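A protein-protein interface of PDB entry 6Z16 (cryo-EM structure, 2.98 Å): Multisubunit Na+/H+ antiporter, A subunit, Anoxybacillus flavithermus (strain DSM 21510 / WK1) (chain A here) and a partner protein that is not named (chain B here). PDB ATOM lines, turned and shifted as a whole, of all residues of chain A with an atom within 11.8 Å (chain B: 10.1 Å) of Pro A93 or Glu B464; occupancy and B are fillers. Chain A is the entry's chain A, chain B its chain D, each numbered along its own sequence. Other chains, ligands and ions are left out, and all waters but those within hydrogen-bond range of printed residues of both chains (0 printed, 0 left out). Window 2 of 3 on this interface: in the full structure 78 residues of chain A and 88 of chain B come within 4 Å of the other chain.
O of Ile B461 sits at hydrogen-bond distance from NE1 of Trp A91 (3.4 Å). The side-chain carboxylate of Glu B464 is in hydrogen-bond range of the side-chain hydroxyl of Ser A94. The side-chain hydroxyl of Ser A94 lies within hydrogen-bond range of the guanidinium group of Arg B467 (3.2 Å). N of Pro A93 lies close to OE1 of Glu B464, at 3.5 Å.
The backbone NH (N) of Trp A91 sits at hydrogen-bond distance from the backbone carbonyl oxygen (O) of Ile A97 (3.0 Å). The backbone NH (N) of Ile A97 is in hydrogen-bond range of the backbone carbonyl oxygen (O) of Ile A92 (2.9 Å). OE2 of Glu B324 lies within salt-bridge range of NE of Arg B467, 3.1 Å away.
Among the printed residues, pairs that only touch across the chains: Ile A92 with Glu B464, Leu A95 with Arg B467, Leu A95 with Ile B390, Ile A92 with Ile B463 and Trp A91 with Gly B460.
Printed residues of chain B within 4 Å of Trp A91: Gly B460 (3.8 Å) and Ile B461 (3.4 Å). Of chain B, only Glu B464 comes within 4 Å of Pro A93. Of the printed residues of chain B, Ser A94 touches Glu B464 (3.3 Å) and Arg B467 (3.2 Å). Of the printed residues of chain B, Leu A95 touches Ile B390 and Arg B467. Met A164 touches none of the printed residues of chain B. Tyr A218 touches none of the printed residues of chain B. Of the printed residues of chain A, Ile B390 touches Leu A95 (3.7 Å). Of the printed residues of chain A, Ile B461 touches Trp A91 (3.4 Å). No residue of chain A comes within 4 Å of Gly B462. Glu B464 touches just these residues of chain A: Ile A92 (3.4 Å), Pro A93 (3.3 Å) and Ser A94 (3.3 Å). No residue of chain A comes within 4 Å of Phe B465. Val B466 touches none of the printed residues of chain A. Arg B467 touches just these residues of chain A: Ser A94 and Leu A95. The nearest residue of chain A that does not touch Glu B464 is Trp A91 (4.1 Å). The nearest printed residue of chain A that does not touch Ile B390 is Ile A97 (4.2 Å).
Hydrophobic or aromatic side chains of chain B that line the printed part of chain A: Ile B390 and Ile B463. Along chain B the printed residues that touch a printed residue of chain A span positions 390 to 467. Of the 17 printed residues of chain A, 5 touch a printed residue of chain B. Among the printed residues, no Asp or Glu carboxylate lies within 4 Å of a Lys or Arg side-chain nitrogen of the other chain.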
ATOM      1  N   THR A  88       1.102 -21.226 -17.750  1.00  0.00           N
ATOM      2  CA  THR A  88      -0.067 -21.290 -18.620  1.00  0.00           C
ATOM      3  C   THR A  88       0.246 -20.617 -19.949  1.00  0.00           C
ATOM      4  O   THR A  88       0.774 -19.505 -19.965  1.00  0.00           O
ATOM      5  CB  THR A  88      -1.270 -20.606 -17.951  1.00  0.00           C
ATOM      6  OG1 THR A  88      -1.537 -21.224 -16.688  1.00  0.00           O
ATOM      7  CG2 THR A  88      -2.513 -20.724 -18.807  1.00  0.00           C
ATOM      8  N   MET A  89      -0.076 -21.287 -21.055  1.00  0.00           N
ATOM      9  CA  MET A  89      -0.005 -20.690 -22.390  1.00  0.00           C
ATOM     10  C   MET A  89      -1.283 -21.026 -23.148  1.00  0.00           C
ATOM     11  O   MET A  89      -1.441 -22.169 -23.605  1.00  0.00           O
ATOM     12  CB  MET A  89       1.211 -21.192 -23.157  1.00  0.00           C
ATOM     13  CG  MET A  89       1.359 -20.573 -24.530  1.00  0.00           C
ATOM     14  SD  MET A  89       2.782 -21.171 -25.458  1.00  0.00           S
ATOM     15  CE  MET A  89       4.118 -20.365 -24.586  1.00  0.00           C
ATOM     16  N   PRO A  90      -2.209 -20.077 -23.308  1.00  0.00           N
ATOM     17  CA  PRO A  90      -3.529 -20.421 -23.858  1.00  0.00           C
ATOM     18  C   PRO A  90      -3.461 -20.722 -25.347  1.00  0.00           C
ATOM     19  O   PRO A  90      -2.685 -20.111 -26.079  1.00  0.00           O
ATOM     20  CB  PRO A  90      -4.362 -19.166 -23.582  1.00  0.00           C
ATOM     21  CG  PRO A  90      -3.366 -18.067 -23.565  1.00  0.00           C
ATOM     22  CD  PRO A  90      -2.109 -18.645 -22.979  1.00  0.00           C
ATOM     23  N   TRP A  91      -4.262 -21.694 -25.794  1.00  0.00           N
ATOM     24  CA  TRP A  91      -4.223 -22.077 -27.197  1.00  0.00           C
ATOM     25  C   TRP A  91      -5.554 -21.865 -27.895  1.00  0.00           C
ATOM     26  O   TRP A  91      -5.589 -21.289 -28.985  1.00  0.00           O
ATOM     27  CB  TRP A  91      -3.770 -23.533 -27.325  1.00  0.00           C
ATOM     28  CG  TRP A  91      -3.689 -24.004 -28.723  1.00  0.00           C
ATOM     29  CD1 TRP A  91      -3.060 -23.382 -29.748  1.00  0.00           C
ATOM     30  CD2 TRP A  91      -4.167 -25.248 -29.240  1.00  0.00           C
ATOM     31  NE1 TRP A  91      -3.159 -24.131 -30.891  1.00  0.00           N
ATOM     32  CE2 TRP A  91      -3.831 -25.288 -30.602  1.00  0.00           C
ATOM     33  CE3 TRP A  91      -4.862 -26.324 -28.688  1.00  0.00           C
ATOM     34  CZ2 TRP A  91      -4.165 -26.357 -31.423  1.00  0.00           C
ATOM     35  CZ3 TRP A  91      -5.196 -27.385 -29.505  1.00  0.00           C
ATOM     36  CH2 TRP A  91      -4.848 -27.394 -30.856  1.00  0.00           C
ATOM     37  N   ILE A  92      -6.653 -22.329 -27.308  1.00  0.00           N
ATOM     38  CA  ILE A  92      -7.994 -21.984 -27.769  1.00  0.00           C
ATOM     39  C   ILE A  92      -8.760 -21.518 -26.538  1.00  0.00           C
ATOM     40  O   ILE A  92      -9.392 -22.340 -25.864  1.00  0.00           O
ATOM     41  CB  ILE A  92      -8.701 -23.173 -28.439  1.00  0.00           C
ATOM     42  CG1 ILE A  92      -7.868 -23.769 -29.565  1.00  0.00           C
ATOM     43  CG2 ILE A  92      -9.993 -22.719 -29.063  1.00  0.00           C
ATOM     44  CD1 ILE A  92      -8.360 -25.100 -30.014  1.00  0.00           C
ATOM     45  N   PRO A  93      -8.710 -20.231 -26.188  1.00  0.00           N
ATOM     46  CA  PRO A  93      -9.300 -19.792 -24.911  1.00  0.00           C
ATOM     47  C   PRO A  93     -10.821 -19.810 -24.868  1.00  0.00           C
ATOM     48  O   PRO A  93     -11.386 -19.823 -23.767  1.00  0.00           O
ATOM     49  CB  PRO A  93      -8.765 -18.364 -24.753  1.00  0.00           C
ATOM     50  CG  PRO A  93      -7.540 -18.329 -25.591  1.00  0.00           C
ATOM     51  CD  PRO A  93      -7.832 -19.202 -26.763  1.00  0.00           C
ATOM     52  N   SER A  94     -11.505 -19.805 -26.009  1.00  0.00           N
ATOM     53  CA  SER A  94     -12.963 -19.850 -25.990  1.00  0.00           C
ATOM     54  C   SER A  94     -13.495 -21.273 -25.888  1.00  0.00           C
ATOM     55  O   SER A  94     -14.572 -21.484 -25.322  1.00  0.00           O
ATOM     56  CB  SER A  94     -13.521 -19.153 -27.225  1.00  0.00           C
ATOM     57  OG  SER A  94     -13.080 -19.802 -28.398  1.00  0.00           O
ATOM     58  N   LEU A  95     -12.773 -22.257 -26.425  1.00  0.00           N
ATOM     59  CA  LEU A  95     -13.048 -23.653 -26.111  1.00  0.00           C
ATOM     60  C   LEU A  95     -12.355 -24.112 -24.843  1.00  0.00           C
ATOM     61  O   LEU A  95     -12.395 -25.314 -24.551  1.00  0.00           O
ATOM     62  CB  LEU A  95     -12.632 -24.575 -27.253  1.00  0.00           C
ATOM     63  CG  LEU A  95     -13.483 -24.526 -28.509  1.00  0.00           C
ATOM     64  CD1 LEU A  95     -12.908 -25.445 -29.550  1.00  0.00           C
ATOM     65  CD2 LEU A  95     -14.904 -24.913 -28.174  1.00  0.00           C
ATOM     66  N   ARG A  96     -11.689 -23.190 -24.136  1.00  0.00           N
ATOM     67  CA  ARG A  96     -11.135 -23.396 -22.799  1.00  0.00           C
ATOM     68  C   ARG A  96     -10.033 -24.461 -22.831  1.00  0.00           C
ATOM     69  O   ARG A  96     -10.057 -25.451 -22.099  1.00  0.00           O
ATOM     70  CB  ARG A  96     -12.263 -23.720 -21.811  1.00  0.00           C
ATOM     71  CG  ARG A  96     -11.977 -23.552 -20.345  1.00  0.00           C
ATOM     72  CD  ARG A  96     -13.269 -23.676 -19.556  1.00  0.00           C
ATOM     73  NE  ARG A  96     -13.892 -24.992 -19.676  1.00  0.00           N
ATOM     74  CZ  ARG A  96     -15.054 -25.215 -20.281  1.00  0.00           C
ATOM     75  NH1 ARG A  96     -15.718 -24.211 -20.834  1.00  0.00           N
ATOM     76  NH2 ARG A  96     -15.550 -26.442 -20.342  1.00  0.00           N
ATOM     77  N   ILE A  97      -9.065 -24.257 -23.725  1.00  0.00           N
ATOM     78  CA  ILE A  97      -7.936 -25.161 -23.907  1.00  0.00           C
ATOM     79  C   ILE A  97      -6.636 -24.367 -23.818  1.00  0.00           C
ATOM     80  O   ILE A  97      -6.450 -23.361 -24.515  1.00  0.00           O
ATOM     81  CB  ILE A  97      -8.025 -25.929 -25.241  1.00  0.00           C
ATOM     82  CG1 ILE A  97      -9.198 -26.904 -25.215  1.00  0.00           C
ATOM     83  CG2 ILE A  97      -6.741 -26.680 -25.541  1.00  0.00           C
ATOM     84  CD1 ILE A  97      -9.466 -27.557 -26.536  1.00  0.00           C
ATOM     85  N   SER A  98      -5.736 -24.821 -22.956  1.00  0.00           N
ATOM     86  CA  SER A  98      -4.442 -24.188 -22.800  1.00  0.00           C
ATOM     87  C   SER A  98      -3.370 -25.263 -22.764  1.00  0.00           C
ATOM     88  O   SER A  98      -3.656 -26.450 -22.615  1.00  0.00           O
ATOM     89  CB  SER A  98      -4.404 -23.337 -21.532  1.00  0.00           C
ATOM     90  OG  SER A  98      -5.349 -22.289 -21.604  1.00  0.00           O
ATOM     91  N   PHE A  99      -2.126 -24.840 -22.940  1.00  0.00           N
ATOM     92  CA  PHE A  99      -0.975 -25.635 -22.542  1.00  0.00           C
ATOM     93  C   PHE A  99      -0.661 -25.216 -21.118  1.00  0.00           C
ATOM     94  O   PHE A  99       0.023 -24.222 -20.875  1.00  0.00           O
ATOM     95  CB  PHE A  99       0.205 -25.406 -23.472  1.00  0.00           C
ATOM     96  CG  PHE A  99       0.013 -25.978 -24.829  1.00  0.00           C
ATOM     97  CD1 PHE A  99       0.216 -27.324 -25.055  1.00  0.00           C
ATOM     98  CD2 PHE A  99      -0.373 -25.174 -25.882  1.00  0.00           C
ATOM     99  CE1 PHE A  99       0.039 -27.861 -26.307  1.00  0.00           C
ATOM    100  CE2 PHE A  99      -0.551 -25.707 -27.141  1.00  0.00           C
ATOM    101  CZ  PHE A  99      -0.344 -27.052 -27.351  1.00  0.00           C
ATOM    102  N   ASP A 100      -1.236 -25.932 -20.164  1.00  0.00           N
ATOM    103  CA  ASP A 100      -0.862 -25.710 -18.783  1.00  0.00           C
ATOM    104  C   ASP A 100       0.387 -26.520 -18.465  1.00  0.00           C
ATOM    105  O   ASP A 100       0.729 -27.480 -19.157  1.00  0.00           O
ATOM    106  CB  ASP A 100      -1.990 -26.103 -17.836  1.00  0.00           C
ATOM    107  CG  ASP A 100      -3.211 -25.238 -17.983  1.00  0.00           C
ATOM    108  OD1 ASP A 100      -3.069 -24.070 -18.383  1.00  0.00           O
ATOM    109  OD2 ASP A 100      -4.320 -25.727 -17.686  1.00  0.00           O
ATOM    110  N   HIS A 158      -3.089 -29.961 -18.479  1.00  0.00           N
ATOM    111  CA  HIS A 158      -4.302 -30.012 -19.275  1.00  0.00           C
ATOM    112  C   HIS A 158      -4.422 -31.393 -19.904  1.00  0.00           C
ATOM    113  O   HIS A 158      -3.416 -31.992 -20.289  1.00  0.00           O
ATOM    114  CB  HIS A 158      -4.255 -28.941 -20.359  1.00  0.00           C
ATOM    115  CG  HIS A 158      -5.549 -28.741 -21.075  1.00  0.00           C
ATOM    116  ND1 HIS A 158      -6.567 -27.967 -20.564  1.00  0.00           N
ATOM    117  CD2 HIS A 158      -5.994 -29.219 -22.259  1.00  0.00           C
ATOM    118  CE1 HIS A 158      -7.576 -27.962 -21.412  1.00  0.00           C
ATOM    119  NE2 HIS A 158      -7.259 -28.722 -22.444  1.00  0.00           N
ATOM    120  N   ILE A 160      -6.169 -32.386 -22.773  1.00  0.00           N
ATOM    121  CA  ILE A 160      -6.042 -32.436 -24.230  1.00  0.00           C
ATOM    122  C   ILE A 160      -4.599 -32.181 -24.651  1.00  0.00           C
ATOM    123  O   ILE A 160      -4.096 -32.806 -25.593  1.00  0.00           O
ATOM    124  CB  ILE A 160      -7.046 -31.461 -24.888  1.00  0.00           C
ATOM    125  CG1 ILE A 160      -8.455 -32.053 -24.874  1.00  0.00           C
ATOM    126  CG2 ILE A 160      -6.684 -31.110 -26.322  1.00  0.00           C
ATOM    127  CD1 ILE A 160      -9.292 -31.695 -23.688  1.00  0.00           C
ATOM    128  N   MET A 164      -2.215 -34.671 -26.710  1.00  0.00           N
ATOM    129  CA  MET A 164      -1.435 -34.229 -27.866  1.00  0.00           C
ATOM    130  C   MET A 164       0.015 -34.692 -27.772  1.00  0.00           C
ATOM    131  O   MET A 164       0.572 -35.254 -28.726  1.00  0.00           O
ATOM    132  CB  MET A 164      -1.493 -32.707 -27.955  1.00  0.00           C
ATOM    133  CG  MET A 164      -0.753 -32.112 -29.132  1.00  0.00           C
ATOM    134  SD  MET A 164      -0.779 -30.316 -29.061  1.00  0.00           S
ATOM    135  CE  MET A 164      -2.504 -29.997 -29.393  1.00  0.00           C
ATOM    136  N   TYR A 218     -11.168 -29.148 -17.218  1.00  0.00           N
ATOM    137  CA  TYR A 218     -10.226 -29.979 -17.948  1.00  0.00           C
ATOM    138  C   TYR A 218      -8.889 -30.137 -17.252  1.00  0.00           C
ATOM    139  O   TYR A 218      -8.137 -31.046 -17.604  1.00  0.00           O
ATOM    140  CB  TYR A 218      -9.929 -29.385 -19.325  1.00  0.00           C
ATOM    141  CG  TYR A 218     -11.058 -29.337 -20.306  1.00  0.00           C
ATOM    142  CD1 TYR A 218     -11.372 -30.436 -21.084  1.00  0.00           C
ATOM    143  CD2 TYR A 218     -11.789 -28.173 -20.481  1.00  0.00           C
ATOM    144  CE1 TYR A 218     -12.391 -30.383 -22.003  1.00  0.00           C
ATOM    145  CE2 TYR A 218     -12.811 -28.108 -21.390  1.00  0.00           C
ATOM    146  CZ  TYR A 218     -13.110 -29.215 -22.148  1.00  0.00           C
ATOM    147  OH  TYR A 218     -14.136 -29.140 -23.056  1.00  0.00           O
ATOM    148  N   HIS B  52     -19.841 -11.771 -41.348  1.00  0.00           N
ATOM    149  CA  HIS B  52     -19.349 -11.719 -39.978  1.00  0.00           C
ATOM    150  C   HIS B  52     -19.623 -10.373 -39.319  1.00  0.00           C
ATOM    151  O   HIS B  52     -19.961 -10.330 -38.132  1.00  0.00           O
ATOM    152  CB  HIS B  52     -17.855 -12.026 -39.939  1.00  0.00           C
ATOM    153  CG  HIS B  52     -17.303 -12.143 -38.553  1.00  0.00           C
ATOM    154  ND1 HIS B  52     -16.814 -11.063 -37.852  1.00  0.00           N
ATOM    155  CD2 HIS B  52     -17.179 -13.210 -37.731  1.00  0.00           C
ATOM    156  CE1 HIS B  52     -16.405 -11.460 -36.662  1.00  0.00           C
ATOM    157  NE2 HIS B  52     -16.615 -12.759 -36.563  1.00  0.00           N
ATOM    158  N   GLU B 324     -21.237 -27.886 -33.878  1.00  0.00           N
ATOM    159  CA  GLU B 324     -19.952 -27.216 -34.023  1.00  0.00           C
ATOM    160  C   GLU B 324     -18.874 -28.181 -34.498  1.00  0.00           C
ATOM    161  O   GLU B 324     -18.109 -27.870 -35.427  1.00  0.00           O
ATOM    162  CB  GLU B 324     -19.589 -26.584 -32.687  1.00  0.00           C
ATOM    163  CG  GLU B 324     -18.397 -25.694 -32.714  1.00  0.00           C
ATOM    164  CD  GLU B 324     -18.218 -24.973 -31.405  1.00  0.00           C
ATOM    165  OE1 GLU B 324     -19.008 -25.226 -30.472  1.00  0.00           O
ATOM    166  OE2 GLU B 324     -17.298 -24.141 -31.311  1.00  0.00           O
ATOM    167  N   PHE B 328     -16.721 -28.031 -38.184  1.00  0.00           N
ATOM    168  CA  PHE B 328     -15.257 -28.101 -38.269  1.00  0.00           C
ATOM    169  C   PHE B 328     -14.794 -29.296 -39.102  1.00  0.00           C
ATOM    170  O   PHE B 328     -13.936 -29.161 -39.998  1.00  0.00           O
ATOM    171  CB  PHE B 328     -14.630 -28.188 -36.874  1.00  0.00           C
ATOM    172  CG  PHE B 328     -14.525 -26.879 -36.147  1.00  0.00           C
ATOM    173  CD1 PHE B 328     -13.579 -25.949 -36.520  1.00  0.00           C
ATOM    174  CD2 PHE B 328     -15.300 -26.619 -35.037  1.00  0.00           C
ATOM    175  CE1 PHE B 328     -13.456 -24.758 -35.845  1.00  0.00           C
ATOM    176  CE2 PHE B 328     -15.184 -25.436 -34.353  1.00  0.00           C
ATOM    177  CZ  PHE B 328     -14.260 -24.503 -34.756  1.00  0.00           C
ATOM    178  N   ILE B 390     -10.272 -31.207 -33.596  1.00  0.00           N
ATOM    179  CA  ILE B 390     -11.246 -30.530 -32.751  1.00  0.00           C
ATOM    180  C   ILE B 390     -12.674 -30.878 -33.158  1.00  0.00           C
ATOM    181  O   ILE B 390     -13.570 -30.900 -32.304  1.00  0.00           O
ATOM    182  CB  ILE B 390     -10.967 -29.011 -32.763  1.00  0.00           C
ATOM    183  CG1 ILE B 390     -11.659 -28.312 -31.598  1.00  0.00           C
ATOM    184  CG2 ILE B 390     -11.358 -28.370 -34.072  1.00  0.00           C
ATOM    185  CD1 ILE B 390     -11.050 -28.639 -30.258  1.00  0.00           C
ATOM    186  N   ALA B 458      -2.283 -24.903 -41.179  1.00  0.00           N
ATOM    187  CA  ALA B 458      -2.635 -23.621 -40.575  1.00  0.00           C
ATOM    188  C   ALA B 458      -4.054 -23.616 -40.031  1.00  0.00           C
ATOM    189  O   ALA B 458      -4.351 -22.879 -39.086  1.00  0.00           O
ATOM    190  CB  ALA B 458      -2.468 -22.503 -41.597  1.00  0.00           C
ATOM    191  N   TYR B 459      -4.940 -24.420 -40.616  1.00  0.00           N
ATOM    192  CA  TYR B 459      -6.279 -24.590 -40.069  1.00  0.00           C
ATOM    193  C   TYR B 459      -6.235 -25.313 -38.735  1.00  0.00           C
ATOM    194  O   TYR B 459      -6.950 -24.941 -37.799  1.00  0.00           O
ATOM    195  CB  TYR B 459      -7.139 -25.351 -41.073  1.00  0.00           C
ATOM    196  CG  TYR B 459      -8.556 -25.594 -40.633  1.00  0.00           C
ATOM    197  CD1 TYR B 459      -9.488 -24.569 -40.629  1.00  0.00           C
ATOM    198  CD2 TYR B 459      -8.970 -26.858 -40.241  1.00  0.00           C
ATOM    199  CE1 TYR B 459     -10.784 -24.793 -40.235  1.00  0.00           C
ATOM    200  CE2 TYR B 459     -10.261 -27.087 -39.842  1.00  0.00           C
ATOM    201  CZ  TYR B 459     -11.162 -26.054 -39.847  1.00  0.00           C
ATOM    202  OH  TYR B 459     -12.452 -26.280 -39.457  1.00  0.00           O
ATOM    203  N   GLY B 460      -5.397 -26.345 -38.631  1.00  0.00           N
ATOM    204  CA  GLY B 460      -5.263 -27.059 -37.373  1.00  0.00           C
ATOM    205  C   GLY B 460      -4.608 -26.243 -36.278  1.00  0.00           C
ATOM    206  O   GLY B 460      -4.965 -26.381 -35.105  1.00  0.00           O
ATOM    207  N   ILE B 461      -3.646 -25.390 -36.636  1.00  0.00           N
ATOM    208  CA  ILE B 461      -3.029 -24.513 -35.644  1.00  0.00           C
ATOM    209  C   ILE B 461      -4.004 -23.424 -35.213  1.00  0.00           C
ATOM    210  O   ILE B 461      -4.227 -23.204 -34.018  1.00  0.00           O
ATOM    211  CB  ILE B 461      -1.729 -23.901 -36.191  1.00  0.00           C
ATOM    212  CG1 ILE B 461      -0.727 -24.989 -36.573  1.00  0.00           C
ATOM    213  CG2 ILE B 461      -1.120 -22.973 -35.169  1.00  0.00           C
ATOM    214  CD1 ILE B 461      -0.314 -25.873 -35.442  1.00  0.00           C
ATOM    215  N   GLY B 462      -4.592 -22.724 -36.174  1.00  0.00           N
ATOM    216  CA  GLY B 462      -5.401 -21.565 -35.870  1.00  0.00           C
ATOM    217  C   GLY B 462      -6.886 -21.804 -35.734  1.00  0.00           C
ATOM    218  O   GLY B 462      -7.670 -21.290 -36.533  1.00  0.00           O
ATOM    219  N   ILE B 463      -7.294 -22.575 -34.726  1.00  0.00           N
ATOM    220  CA  ILE B 463      -8.715 -22.779 -34.468  1.00  0.00           C
ATOM    221  C   ILE B 463      -9.335 -21.523 -33.867  1.00  0.00           C
ATOM    222  O   ILE B 463     -10.511 -21.228 -34.105  1.00  0.00           O
ATOM    223  CB  ILE B 463      -8.894 -24.023 -33.570  1.00  0.00           C
ATOM    224  CG1 ILE B 463      -8.386 -25.275 -34.280  1.00  0.00           C
ATOM    225  CG2 ILE B 463     -10.341 -24.259 -33.162  1.00  0.00           C
ATOM    226  CD1 ILE B 463      -9.184 -25.634 -35.507  1.00  0.00           C
ATOM    227  N   GLU B 464      -8.555 -20.736 -33.128  1.00  0.00           N
ATOM    228  CA  GLU B 464      -9.099 -19.553 -32.467  1.00  0.00           C
ATOM    229  C   GLU B 464      -9.436 -18.444 -33.462  1.00  0.00           C
ATOM    230  O   GLU B 464     -10.345 -17.645 -33.214  1.00  0.00           O
ATOM    231  CB  GLU B 464      -8.110 -19.069 -31.401  1.00  0.00           C
ATOM    232  CG  GLU B 464      -8.542 -17.874 -30.564  1.00  0.00           C
ATOM    233  CD  GLU B 464      -9.744 -18.155 -29.686  1.00  0.00           C
ATOM    234  OE1 GLU B 464      -9.976 -19.325 -29.322  1.00  0.00           O
ATOM    235  OE2 GLU B 464     -10.459 -17.191 -29.345  1.00  0.00           O
ATOM    236  N   PHE B 465      -8.744 -18.396 -34.600  1.00  0.00           N
ATOM    237  CA  PHE B 465      -9.135 -17.475 -35.663  1.00  0.00           C
ATOM    238  C   PHE B 465     -10.426 -17.927 -36.332  1.00  0.00           C
ATOM    239  O   PHE B 465     -11.380 -17.152 -36.450  1.00  0.00           O
ATOM    240  CB  PHE B 465      -8.008 -17.355 -36.691  1.00  0.00           C
ATOM    241  CG  PHE B 465      -8.333 -16.454 -37.854  1.00  0.00           C
ATOM    242  CD1 PHE B 465      -8.403 -15.079 -37.690  1.00  0.00           C
ATOM    243  CD2 PHE B 465      -8.549 -16.982 -39.118  1.00  0.00           C
ATOM    244  CE1 PHE B 465      -8.701 -14.254 -38.757  1.00  0.00           C
ATOM    245  CE2 PHE B 465      -8.842 -16.163 -40.187  1.00  0.00           C
ATOM    246  CZ  PHE B 465      -8.918 -14.798 -40.004  1.00  0.00           C
ATOM    247  N   VAL B 466     -10.482 -19.197 -36.747  1.00  0.00           N
ATOM    248  CA  VAL B 466     -11.593 -19.706 -37.549  1.00  0.00           C
ATOM    249  C   VAL B 466     -12.791 -20.111 -36.702  1.00  0.00           C
ATOM    250  O   VAL B 466     -13.809 -20.549 -37.247  1.00  0.00           O
ATOM    251  CB  VAL B 466     -11.035 -20.859 -38.416  1.00  0.00           C
ATOM    252  CG1 VAL B 466     -10.868 -22.122 -37.613  1.00  0.00           C
ATOM    253  CG2 VAL B 466     -11.844 -21.090 -39.692  1.00  0.00           C
ATOM    254  N   ARG B 467     -12.727 -19.949 -35.392  1.00  0.00           N
ATOM    255  CA  ARG B 467     -13.866 -20.364 -34.578  1.00  0.00           C
ATOM    256  C   ARG B 467     -15.061 -19.398 -34.538  1.00  0.00           C
ATOM    257  O   ARG B 467     -16.180 -19.902 -34.662  1.00  0.00           O
ATOM    258  CB  ARG B 467     -13.426 -20.693 -33.147  1.00  0.00           C
ATOM    259  CG  ARG B 467     -14.556 -21.287 -32.312  1.00  0.00           C
ATOM    260  CD  ARG B 467     -14.181 -21.579 -30.894  1.00  0.00           C
ATOM    261  NE  ARG B 467     -15.320 -22.098 -30.143  1.00  0.00           N
ATOM    262  CZ  ARG B 467     -16.201 -21.340 -29.501  1.00  0.00           C
ATOM    263  NH1 ARG B 467     -16.078 -20.023 -29.516  1.00  0.00           N
ATOM    264  NH2 ARG B 467     -17.207 -21.895 -28.845  1.00  0.00           N
ATOM    265  N   PRO B 468     -14.933 -18.061 -34.368  1.00  0.00           N
ATOM    266  CA  PRO B 468     -16.158 -17.234 -34.227  1.00  0.00           C
ATOM    267  C   PRO B 468     -17.078 -17.208 -35.446  1.00  0.00           C
ATOM    268  O   PRO B 468     -18.290 -16.986 -35.279  1.00  0.00           O
ATOM    269  CB  PRO B 468     -15.608 -15.836 -33.925  1.00  0.00           C
ATOM    270  CG  PRO B 468     -14.303 -16.072 -33.348  1.00  0.00           C
ATOM    271  CD  PRO B 468     -13.746 -17.226 -34.087  1.00  0.00           C
ATOM    272  N   PHE B 469     -16.556 -17.486 -36.644  1.00  0.00           N
ATOM    273  CA  PHE B 469     -17.413 -17.756 -37.792  1.00  0.00           C
ATOM    274  C   PHE B 469     -18.287 -18.977 -37.538  1.00  0.00           C
ATOM    275  O   PHE B 469     -19.506 -18.944 -37.750  1.00  0.00           O
ATOM    276  CB  PHE B 469     -16.566 -17.982 -39.043  1.00  0.00           C
ATOM    277  CG  PHE B 469     -15.686 -16.829 -39.400  1.00  0.00           C
ATOM    278  CD1 PHE B 469     -16.212 -15.684 -39.965  1.00  0.00           C
ATOM    279  CD2 PHE B 469     -14.320 -16.910 -39.210  1.00  0.00           C
ATOM    280  CE1 PHE B 469     -15.394 -14.626 -40.301  1.00  0.00           C
ATOM    281  CE2 PHE B 469     -13.498 -15.857 -39.548  1.00  0.00           C
ATOM    282  CZ  PHE B 469     -14.037 -14.714 -40.092  1.00  0.00           C
ATOM    283  N   VAL B 470     -17.673 -20.058 -37.050  1.00  0.00           N
ATOM    284  CA  VAL B 470     -18.398 -21.287 -36.751  1.00  0.00           C
ATOM    285  C   VAL B 470     -19.346 -21.078 -35.576  1.00  0.00           C
ATOM    286  O   VAL B 470     -20.416 -21.688 -35.521  1.00  0.00           O
ATOM    287  CB  VAL B 470     -17.380 -22.421 -36.511  1.00  0.00           C
ATOM    288  CG1 VAL B 470     -18.057 -23.733 -36.196  1.00  0.00           C
ATOM    289  CG2 VAL B 470     -16.495 -22.580 -37.725  1.00  0.00           C
ATOM    290  N   LEU B 471     -19.017 -20.164 -34.666  1.00  0.00           N
ATOM    291  CA  LEU B 471     -19.916 -19.862 -33.558  1.00  0.00           C
ATOM    292  C   LEU B 471     -21.170 -19.144 -34.039  1.00  0.00           C
ATOM    293  O   LEU B 471     -22.276 -19.447 -33.578  1.00  0.00           O
ATOM    294  CB  LEU B 471     -19.196 -19.031 -32.501  1.00  0.00           C
ATOM    295  CG  LEU B 471     -20.040 -18.693 -31.273  1.00  0.00           C
ATOM    296  CD1 LEU B 471     -20.452 -19.961 -30.559  1.00  0.00           C
ATOM    297  CD2 LEU B 471     -19.296 -17.760 -30.342  1.00  0.00           C
